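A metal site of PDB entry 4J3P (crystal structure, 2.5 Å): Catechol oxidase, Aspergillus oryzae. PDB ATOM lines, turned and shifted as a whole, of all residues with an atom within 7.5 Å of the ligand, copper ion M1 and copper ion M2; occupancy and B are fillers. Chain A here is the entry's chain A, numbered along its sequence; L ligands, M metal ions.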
ATOM      1  N   HIS A 102       5.721   2.150  21.741  1.00  0.00           N
ATOM      2  CA  HIS A 102       5.804   3.503  21.222  1.00  0.00           C
ATOM      3  C   HIS A 102       7.209   3.813  20.721  1.00  0.00           C
ATOM      4  O   HIS A 102       7.373   4.383  19.641  1.00  0.00           O
ATOM      5  CB  HIS A 102       5.401   4.522  22.273  1.00  0.00           C
ATOM      6  CG  HIS A 102       5.170   5.889  21.717  1.00  0.00           C
ATOM      7  ND1 HIS A 102       6.194   6.798  21.545  1.00  0.00           N
ATOM      8  CD2 HIS A 102       4.051   6.492  21.268  1.00  0.00           C
ATOM      9  CE1 HIS A 102       5.703   7.907  21.016  1.00  0.00           C
ATOM     10  NE2 HIS A 102       4.399   7.754  20.845  1.00  0.00           N
ATOM     11  N   GLN A 105       7.907   2.046  17.414  1.00  0.00           N
ATOM     12  CA  GLN A 105       7.215   2.433  16.201  1.00  0.00           C
ATOM     13  C   GLN A 105       7.247   3.934  15.921  1.00  0.00           C
ATOM     14  O   GLN A 105       6.533   4.411  15.048  1.00  0.00           O
ATOM     15  CB  GLN A 105       5.760   1.954  16.245  1.00  0.00           C
ATOM     16  CG  GLN A 105       5.596   0.461  16.466  1.00  0.00           C
ATOM     17  CD  GLN A 105       4.170   0.002  16.298  1.00  0.00           C
ATOM     18  OE1 GLN A 105       3.593   0.155  15.231  1.00  0.00           O
ATOM     19  NE2 GLN A 105       3.588  -0.546  17.352  1.00  0.00           N
ATOM     20  N   THR A 106       8.056   4.669  16.683  1.00  0.00           N
ATOM     21  CA  THR A 106       8.097   6.141  16.576  1.00  0.00           C
ATOM     22  C   THR A 106       8.244   6.629  15.141  1.00  0.00           C
ATOM     23  O   THR A 106       7.594   7.598  14.741  1.00  0.00           O
ATOM     24  CB  THR A 106       9.232   6.730  17.479  1.00  0.00           C
ATOM     25  OG1 THR A 106       8.800   6.697  18.847  1.00  0.00           O
ATOM     26  CG2 THR A 106       9.564   8.180  17.113  1.00  0.00           C
ATOM     27  N   ILE A 109       4.824   6.512  13.221  1.00  0.00           N
ATOM     28  CA  ILE A 109       3.605   6.998  13.866  1.00  0.00           C
ATOM     29  C   ILE A 109       3.585   8.499  14.121  1.00  0.00           C
ATOM     30  O   ILE A 109       2.636   9.026  14.683  1.00  0.00           O
ATOM     31  CB  ILE A 109       3.292   6.282  15.202  1.00  0.00           C
ATOM     32  CG1 ILE A 109       4.384   6.588  16.233  1.00  0.00           C
ATOM     33  CG2 ILE A 109       3.105   4.778  14.982  1.00  0.00           C
ATOM     34  CD1 ILE A 109       4.258   5.783  17.521  1.00  0.00           C
ATOM     35  N   HIS A 110       4.643   9.193  13.705  1.00  0.00           N
ATOM     36  CA  HIS A 110       4.614  10.645  13.802  1.00  0.00           C
ATOM     37  C   HIS A 110       4.874  11.203  12.433  1.00  0.00           C
ATOM     38  O   HIS A 110       5.637  10.617  11.670  1.00  0.00           O
ATOM     39  CB  HIS A 110       5.605  11.136  14.858  1.00  0.00           C
ATOM     40  CG  HIS A 110       5.330  10.598  16.227  1.00  0.00           C
ATOM     41  ND1 HIS A 110       5.953   9.481  16.724  1.00  0.00           N
ATOM     42  CD2 HIS A 110       4.457  11.005  17.188  1.00  0.00           C
ATOM     43  CE1 HIS A 110       5.490   9.224  17.945  1.00  0.00           C
ATOM     44  NE2 HIS A 110       4.582  10.132  18.237  1.00  0.00           N
ATOM     45  N   PHE A 115      -0.738   9.013  12.129  1.00  0.00           N
ATOM     46  CA  PHE A 115      -0.465   9.681  13.394  1.00  0.00           C
ATOM     47  C   PHE A 115      -1.660   9.748  14.330  1.00  0.00           C
ATOM     48  O   PHE A 115      -1.631   9.227  15.448  1.00  0.00           O
ATOM     49  CB  PHE A 115       0.063  11.085  13.146  1.00  0.00           C
ATOM     50  CG  PHE A 115       0.063  11.945  14.369  1.00  0.00           C
ATOM     51  CD1 PHE A 115       0.875  11.626  15.453  1.00  0.00           C
ATOM     52  CD2 PHE A 115      -0.737  13.066  14.451  1.00  0.00           C
ATOM     53  CE1 PHE A 115       0.881  12.413  16.580  1.00  0.00           C
ATOM     54  CE2 PHE A 115      -0.724  13.862  15.587  1.00  0.00           C
ATOM     55  CZ  PHE A 115       0.083  13.540  16.654  1.00  0.00           C
ATOM     56  N   TRP A 118      -3.500   6.226  15.098  1.00  0.00           N
ATOM     57  CA  TRP A 118      -2.685   5.273  15.840  1.00  0.00           C
ATOM     58  C   TRP A 118      -2.748   5.673  17.318  1.00  0.00           C
ATOM     59  O   TRP A 118      -2.973   4.845  18.204  1.00  0.00           O
ATOM     60  CB  TRP A 118      -1.229   5.268  15.317  1.00  0.00           C
ATOM     61  CG  TRP A 118      -0.319   4.267  16.003  1.00  0.00           C
ATOM     62  CD1 TRP A 118       0.074   3.041  15.549  1.00  0.00           C
ATOM     63  CD2 TRP A 118       0.310   4.426  17.292  1.00  0.00           C
ATOM     64  NE1 TRP A 118       0.903   2.426  16.450  1.00  0.00           N
ATOM     65  CE2 TRP A 118       1.056   3.257  17.537  1.00  0.00           C
ATOM     66  CE3 TRP A 118       0.300   5.429  18.252  1.00  0.00           C
ATOM     67  CZ2 TRP A 118       1.790   3.070  18.698  1.00  0.00           C
ATOM     68  CZ3 TRP A 118       1.037   5.254  19.398  1.00  0.00           C
ATOM     69  CH2 TRP A 118       1.761   4.078  19.620  1.00  0.00           C
ATOM     70  N   HIS A 119      -2.578   6.965  17.585  1.00  0.00           N
ATOM     71  CA  HIS A 119      -2.617   7.438  18.957  1.00  0.00           C
ATOM     72  C   HIS A 119      -3.979   7.259  19.596  1.00  0.00           C
ATOM     73  O   HIS A 119      -4.078   6.887  20.771  1.00  0.00           O
ATOM     74  CB  HIS A 119      -2.125   8.880  19.056  1.00  0.00           C
ATOM     75  CG  HIS A 119      -0.632   8.988  18.969  1.00  0.00           C
ATOM     76  ND1 HIS A 119       0.046   8.877  17.779  1.00  0.00           N
ATOM     77  CD2 HIS A 119       0.305   9.147  19.942  1.00  0.00           C
ATOM     78  CE1 HIS A 119       1.345   8.995  18.012  1.00  0.00           C
ATOM     79  NE2 HIS A 119       1.525   9.162  19.311  1.00  0.00           N
ATOM     80  N   PHE A 122      -3.990   3.795  20.510  1.00  0.00           N
ATOM     81  CA  PHE A 122      -2.997   3.623  21.578  1.00  0.00           C
ATOM     82  C   PHE A 122      -3.589   3.950  22.944  1.00  0.00           C
ATOM     83  O   PHE A 122      -3.475   3.159  23.888  1.00  0.00           O
ATOM     84  CB  PHE A 122      -1.773   4.498  21.289  1.00  0.00           C
ATOM     85  CG  PHE A 122      -0.595   4.203  22.152  1.00  0.00           C
ATOM     86  CD1 PHE A 122      -0.134   2.916  22.324  1.00  0.00           C
ATOM     87  CD2 PHE A 122       0.083   5.237  22.778  1.00  0.00           C
ATOM     88  CE1 PHE A 122       0.966   2.649  23.117  1.00  0.00           C
ATOM     89  CE2 PHE A 122       1.190   4.986  23.572  1.00  0.00           C
ATOM     90  CZ  PHE A 122       1.631   3.688  23.745  1.00  0.00           C
ATOM     91  N   HIS A 284       0.601  20.036  19.911  1.00  0.00           N
ATOM     92  CA  HIS A 284       1.138  18.711  20.223  1.00  0.00           C
ATOM     93  C   HIS A 284       2.568  18.725  20.723  1.00  0.00           C
ATOM     94  O   HIS A 284       2.895  18.039  21.676  1.00  0.00           O
ATOM     95  CB  HIS A 284       1.032  17.756  19.046  1.00  0.00           C
ATOM     96  CG  HIS A 284       1.650  16.434  19.313  1.00  0.00           C
ATOM     97  ND1 HIS A 284       2.844  16.037  18.747  1.00  0.00           N
ATOM     98  CD2 HIS A 284       1.268  15.410  20.115  1.00  0.00           C
ATOM     99  CE1 HIS A 284       3.155  14.827  19.173  1.00  0.00           C
ATOM    100  NE2 HIS A 284       2.219  14.425  20.016  1.00  0.00           N
ATOM    101  N   GLY A 285       3.442  19.482  20.062  1.00  0.00           N
ATOM    102  CA  GLY A 285       4.815  19.572  20.494  1.00  0.00           C
ATOM    103  C   GLY A 285       4.862  20.441  21.734  1.00  0.00           C
ATOM    104  O   GLY A 285       5.669  20.224  22.652  1.00  0.00           O
ATOM    105  N   HIS A 288       3.852  18.247  24.912  1.00  0.00           N
ATOM    106  CA  HIS A 288       4.972  17.382  25.267  1.00  0.00           C
ATOM    107  C   HIS A 288       6.142  18.163  25.903  1.00  0.00           C
ATOM    108  O   HIS A 288       6.547  17.870  27.019  1.00  0.00           O
ATOM    109  CB  HIS A 288       5.494  16.646  24.025  1.00  0.00           C
ATOM    110  CG  HIS A 288       4.636  15.503  23.600  1.00  0.00           C
ATOM    111  ND1 HIS A 288       4.494  14.353  24.348  1.00  0.00           N
ATOM    112  CD2 HIS A 288       3.898  15.320  22.478  1.00  0.00           C
ATOM    113  CE1 HIS A 288       3.692  13.517  23.714  1.00  0.00           C
ATOM    114  NE2 HIS A 288       3.317  14.078  22.574  1.00  0.00           N
ATOM    115  N   ASP A 298      11.707  13.583  24.833  1.00  0.00           N
ATOM    116  CA  ASP A 298      12.101  12.472  23.979  1.00  0.00           C
ATOM    117  C   ASP A 298      10.884  11.971  23.195  1.00  0.00           C
ATOM    118  O   ASP A 298      10.046  11.240  23.714  1.00  0.00           O
ATOM    119  CB  ASP A 298      12.711  11.339  24.822  1.00  0.00           C
ATOM    120  CG  ASP A 298      13.263  10.193  23.971  1.00  0.00           C
ATOM    121  OD1 ASP A 298      12.547   9.690  23.090  1.00  0.00           O
ATOM    122  OD2 ASP A 298      14.406   9.764  24.227  1.00  0.00           O
ATOM    123  N   VAL A 299      10.826  12.376  21.926  1.00  0.00           N
ATOM    124  CA  VAL A 299       9.772  11.987  21.017  1.00  0.00           C
ATOM    125  C   VAL A 299       9.482  10.479  20.994  1.00  0.00           C
ATOM    126  O   VAL A 299       8.346  10.075  20.771  1.00  0.00           O
ATOM    127  CB  VAL A 299      10.068  12.526  19.588  1.00  0.00           C
ATOM    128  CG1 VAL A 299       9.306  11.757  18.535  1.00  0.00           C
ATOM    129  CG2 VAL A 299       9.770  14.019  19.509  1.00  0.00           C
ATOM    130  N   TYR A 300      10.482   9.645  21.247  1.00  0.00           N
ATOM    131  CA  TYR A 300      10.288   8.199  21.254  1.00  0.00           C
ATOM    132  C   TYR A 300       9.694   7.690  22.559  1.00  0.00           C
ATOM    133  O   TYR A 300       8.864   6.787  22.552  1.00  0.00           O
ATOM    134  CB  TYR A 300      11.613   7.448  21.066  1.00  0.00           C
ATOM    135  CG  TYR A 300      12.341   7.635  19.750  1.00  0.00           C
ATOM    136  CD1 TYR A 300      12.538   6.558  18.884  1.00  0.00           C
ATOM    137  CD2 TYR A 300      12.870   8.854  19.393  1.00  0.00           C
ATOM    138  CE1 TYR A 300      13.231   6.708  17.687  1.00  0.00           C
ATOM    139  CE2 TYR A 300      13.545   9.031  18.201  1.00  0.00           C
ATOM    140  CZ  TYR A 300      13.725   7.948  17.353  1.00  0.00           C
ATOM    141  OH  TYR A 300      14.421   8.146  16.182  1.00  0.00           O
ATOM    142  N   VAL A 301      10.179   8.240  23.666  1.00  0.00           N
ATOM    143  CA  VAL A 301       9.912   7.650  24.982  1.00  0.00           C
ATOM    144  C   VAL A 301       8.805   8.402  25.733  1.00  0.00           C
ATOM    145  O   VAL A 301       8.453   8.043  26.855  1.00  0.00           O
ATOM    146  CB  VAL A 301      11.213   7.606  25.812  1.00  0.00           C
ATOM    147  CG1 VAL A 301      11.067   6.693  27.035  1.00  0.00           C
ATOM    148  CG2 VAL A 301      12.344   7.092  24.946  1.00  0.00           C
ATOM    149  N   SER A 302       8.229   9.399  25.084  1.00  0.00           N
ATOM    150  CA  SER A 302       7.234  10.259  25.736  1.00  0.00           C
ATOM    151  C   SER A 302       6.116   9.586  26.546  1.00  0.00           C
ATOM    152  O   SER A 302       5.665  10.154  27.537  1.00  0.00           O
ATOM    153  CB  SER A 302       6.653  11.249  24.744  1.00  0.00           C
ATOM    154  OG  SER A 302       6.156  10.573  23.623  1.00  0.00           O
ATOM    155  N   PRO A 303       5.647   8.389  26.155  1.00  0.00           N
ATOM    156  CA  PRO A 303       4.628   7.775  27.019  1.00  0.00           C
ATOM    157  C   PRO A 303       5.149   7.397  28.401  1.00  0.00           C
ATOM    158  O   PRO A 303       4.361   7.076  29.298  1.00  0.00           O
ATOM    159  CB  PRO A 303       4.247   6.504  26.273  1.00  0.00           C
ATOM    160  CG  PRO A 303       4.619   6.737  24.898  1.00  0.00           C
ATOM    161  CD  PRO A 303       5.819   7.623  24.911  1.00  0.00           C
ATOM    162  N   PHE A 308       1.340  12.015  29.469  1.00  0.00           N
ATOM    163  CA  PHE A 308       1.148  11.663  28.072  1.00  0.00           C
ATOM    164  C   PHE A 308      -0.297  11.286  27.758  1.00  0.00           C
ATOM    165  O   PHE A 308      -0.867  11.742  26.767  1.00  0.00           O
ATOM    166  CB  PHE A 308       2.066  10.487  27.722  1.00  0.00           C
ATOM    167  CG  PHE A 308       1.892   9.959  26.343  1.00  0.00           C
ATOM    168  CD1 PHE A 308       0.984   8.924  26.085  1.00  0.00           C
ATOM    169  CD2 PHE A 308       2.644  10.467  25.289  1.00  0.00           C
ATOM    170  CE1 PHE A 308       0.818   8.430  24.812  1.00  0.00           C
ATOM    171  CE2 PHE A 308       2.483   9.972  24.003  1.00  0.00           C
ATOM    172  CZ  PHE A 308       1.568   8.951  23.757  1.00  0.00           C
ATOM    173  N   HIS A 311      -2.590  14.399  27.850  1.00  0.00           N
ATOM    174  CA  HIS A 311      -2.177  15.173  26.684  1.00  0.00           C
ATOM    175  C   HIS A 311      -2.813  14.589  25.416  1.00  0.00           C
ATOM    176  O   HIS A 311      -3.452  15.287  24.631  1.00  0.00           O
ATOM    177  CB  HIS A 311      -0.649  15.189  26.582  1.00  0.00           C
ATOM    178  CG  HIS A 311      -0.124  15.883  25.360  1.00  0.00           C
ATOM    179  ND1 HIS A 311      -0.410  17.199  25.077  1.00  0.00           N
ATOM    180  CD2 HIS A 311       0.673  15.443  24.359  1.00  0.00           C
ATOM    181  CE1 HIS A 311       0.195  17.544  23.954  1.00  0.00           C
ATOM    182  NE2 HIS A 311       0.856  16.500  23.492  1.00  0.00           N
ATOM    183  N   HIS A 312      -2.651  13.292  25.223  1.00  0.00           N
ATOM    184  CA  HIS A 312      -3.186  12.684  24.019  1.00  0.00           C
ATOM    185  C   HIS A 312      -4.679  12.463  24.081  1.00  0.00           C
ATOM    186  O   HIS A 312      -5.309  12.224  23.052  1.00  0.00           O
ATOM    187  CB  HIS A 312      -2.422  11.421  23.635  1.00  0.00           C
ATOM    188  CG  HIS A 312      -1.232  11.714  22.780  1.00  0.00           C
ATOM    189  ND1 HIS A 312      -1.295  11.747  21.405  1.00  0.00           N
ATOM    190  CD2 HIS A 312       0.034  12.039  23.107  1.00  0.00           C
ATOM    191  CE1 HIS A 312      -0.101  12.051  20.923  1.00  0.00           C
ATOM    192  NE2 HIS A 312       0.717  12.242  21.939  1.00  0.00           N
ATOM    193  N   ILE A 315      -5.501  15.660  22.505  1.00  0.00           N
ATOM    194  CA  ILE A 315      -5.167  15.614  21.093  1.00  0.00           C
ATOM    195  C   ILE A 315      -6.294  14.936  20.340  1.00  0.00           C
ATOM    196  O   ILE A 315      -6.774  15.429  19.319  1.00  0.00           O
ATOM    197  CB  ILE A 315      -3.874  14.793  20.856  1.00  0.00           C
ATOM    198  CG1 ILE A 315      -2.649  15.508  21.437  1.00  0.00           C
ATOM    199  CG2 ILE A 315      -3.700  14.507  19.363  1.00  0.00           C
ATOM    200  CD1 ILE A 315      -2.275  16.787  20.695  1.00  0.00           C
HETATM  201  O1  LIG L   1       4.482  11.336  20.715  1.00  0.00           O
HETATM  202  O2  LIG L   1       3.369  10.923  20.555  1.00  0.00           O
HETATM  203 CU    CU M   1       2.520  12.863  21.389  1.00  0.00          CU
HETATM  204 CU    CU M   2       3.502   9.088  19.756  1.00  0.00          CU
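Phe 308 touches the ligand.
Hydrophobic or aromatic side chains that line the ligand: His 102, His 110, His 119, His 288, Phe 308 and His 312.
Of the 22 residues printed, 8 come within 4 Å of the ligand.
The nearest printed residue that does not touch the ligand is Val 299 (4.1 Å).
The side-chain hydroxyl (OG) of Ser 302 lies close to an oxygen (O1) of the ligand, at 3.4 Å.
NE2 of His 288 binds copper ion M1, at 1.9 Å.
NE2 of His 312 is bound to copper ion M1 (2.0 Å).
NE2 of His 284 is bound to copper ion M1 (2.1 Å).
O2 of the ligand binds copper ion M1 (2.3 Å).
Copper ion M1 has four donor atoms within binding distance.
Merely in contact with copper ion M1: Phe 308 (3.9 Å).
Within 4 Å of copper ion M1: His 284, His 288, Phe 308 and His 312.
The nearest printed residue that does not touch copper ion M1 is His 311 (4.3 Å).
Copper ion M2 is bound by NE2 of His 102 (1.9 Å), O2 of the ligand (2.0 Å), NE2 of His 119 (2.0 Å) and NE2 of His 110 (2.1 Å).
O of His 102 sits at hydrogen-bond distance from OG1 of Thr 106 (2.8 Å).
The backbone carbonyl oxygen (O) of Tyr 300 is in hydrogen-bond range of a ring nitrogen (ND1) of His 102 (2.9 Å).
The backbone carbonyl oxygen (O) of Phe 115 sits at hydrogen-bond distance from a ring nitrogen (ND1) of His 119 (2.9 Å).
O of His 284 lies within hydrogen-bond range of NE2 of His 311 (3.1 Å).
The backbone carbonyl oxygen (O) of Thr 106 lies within hydrogen-bond range of a ring nitrogen (ND1) of His 110, 3.2 Å away.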
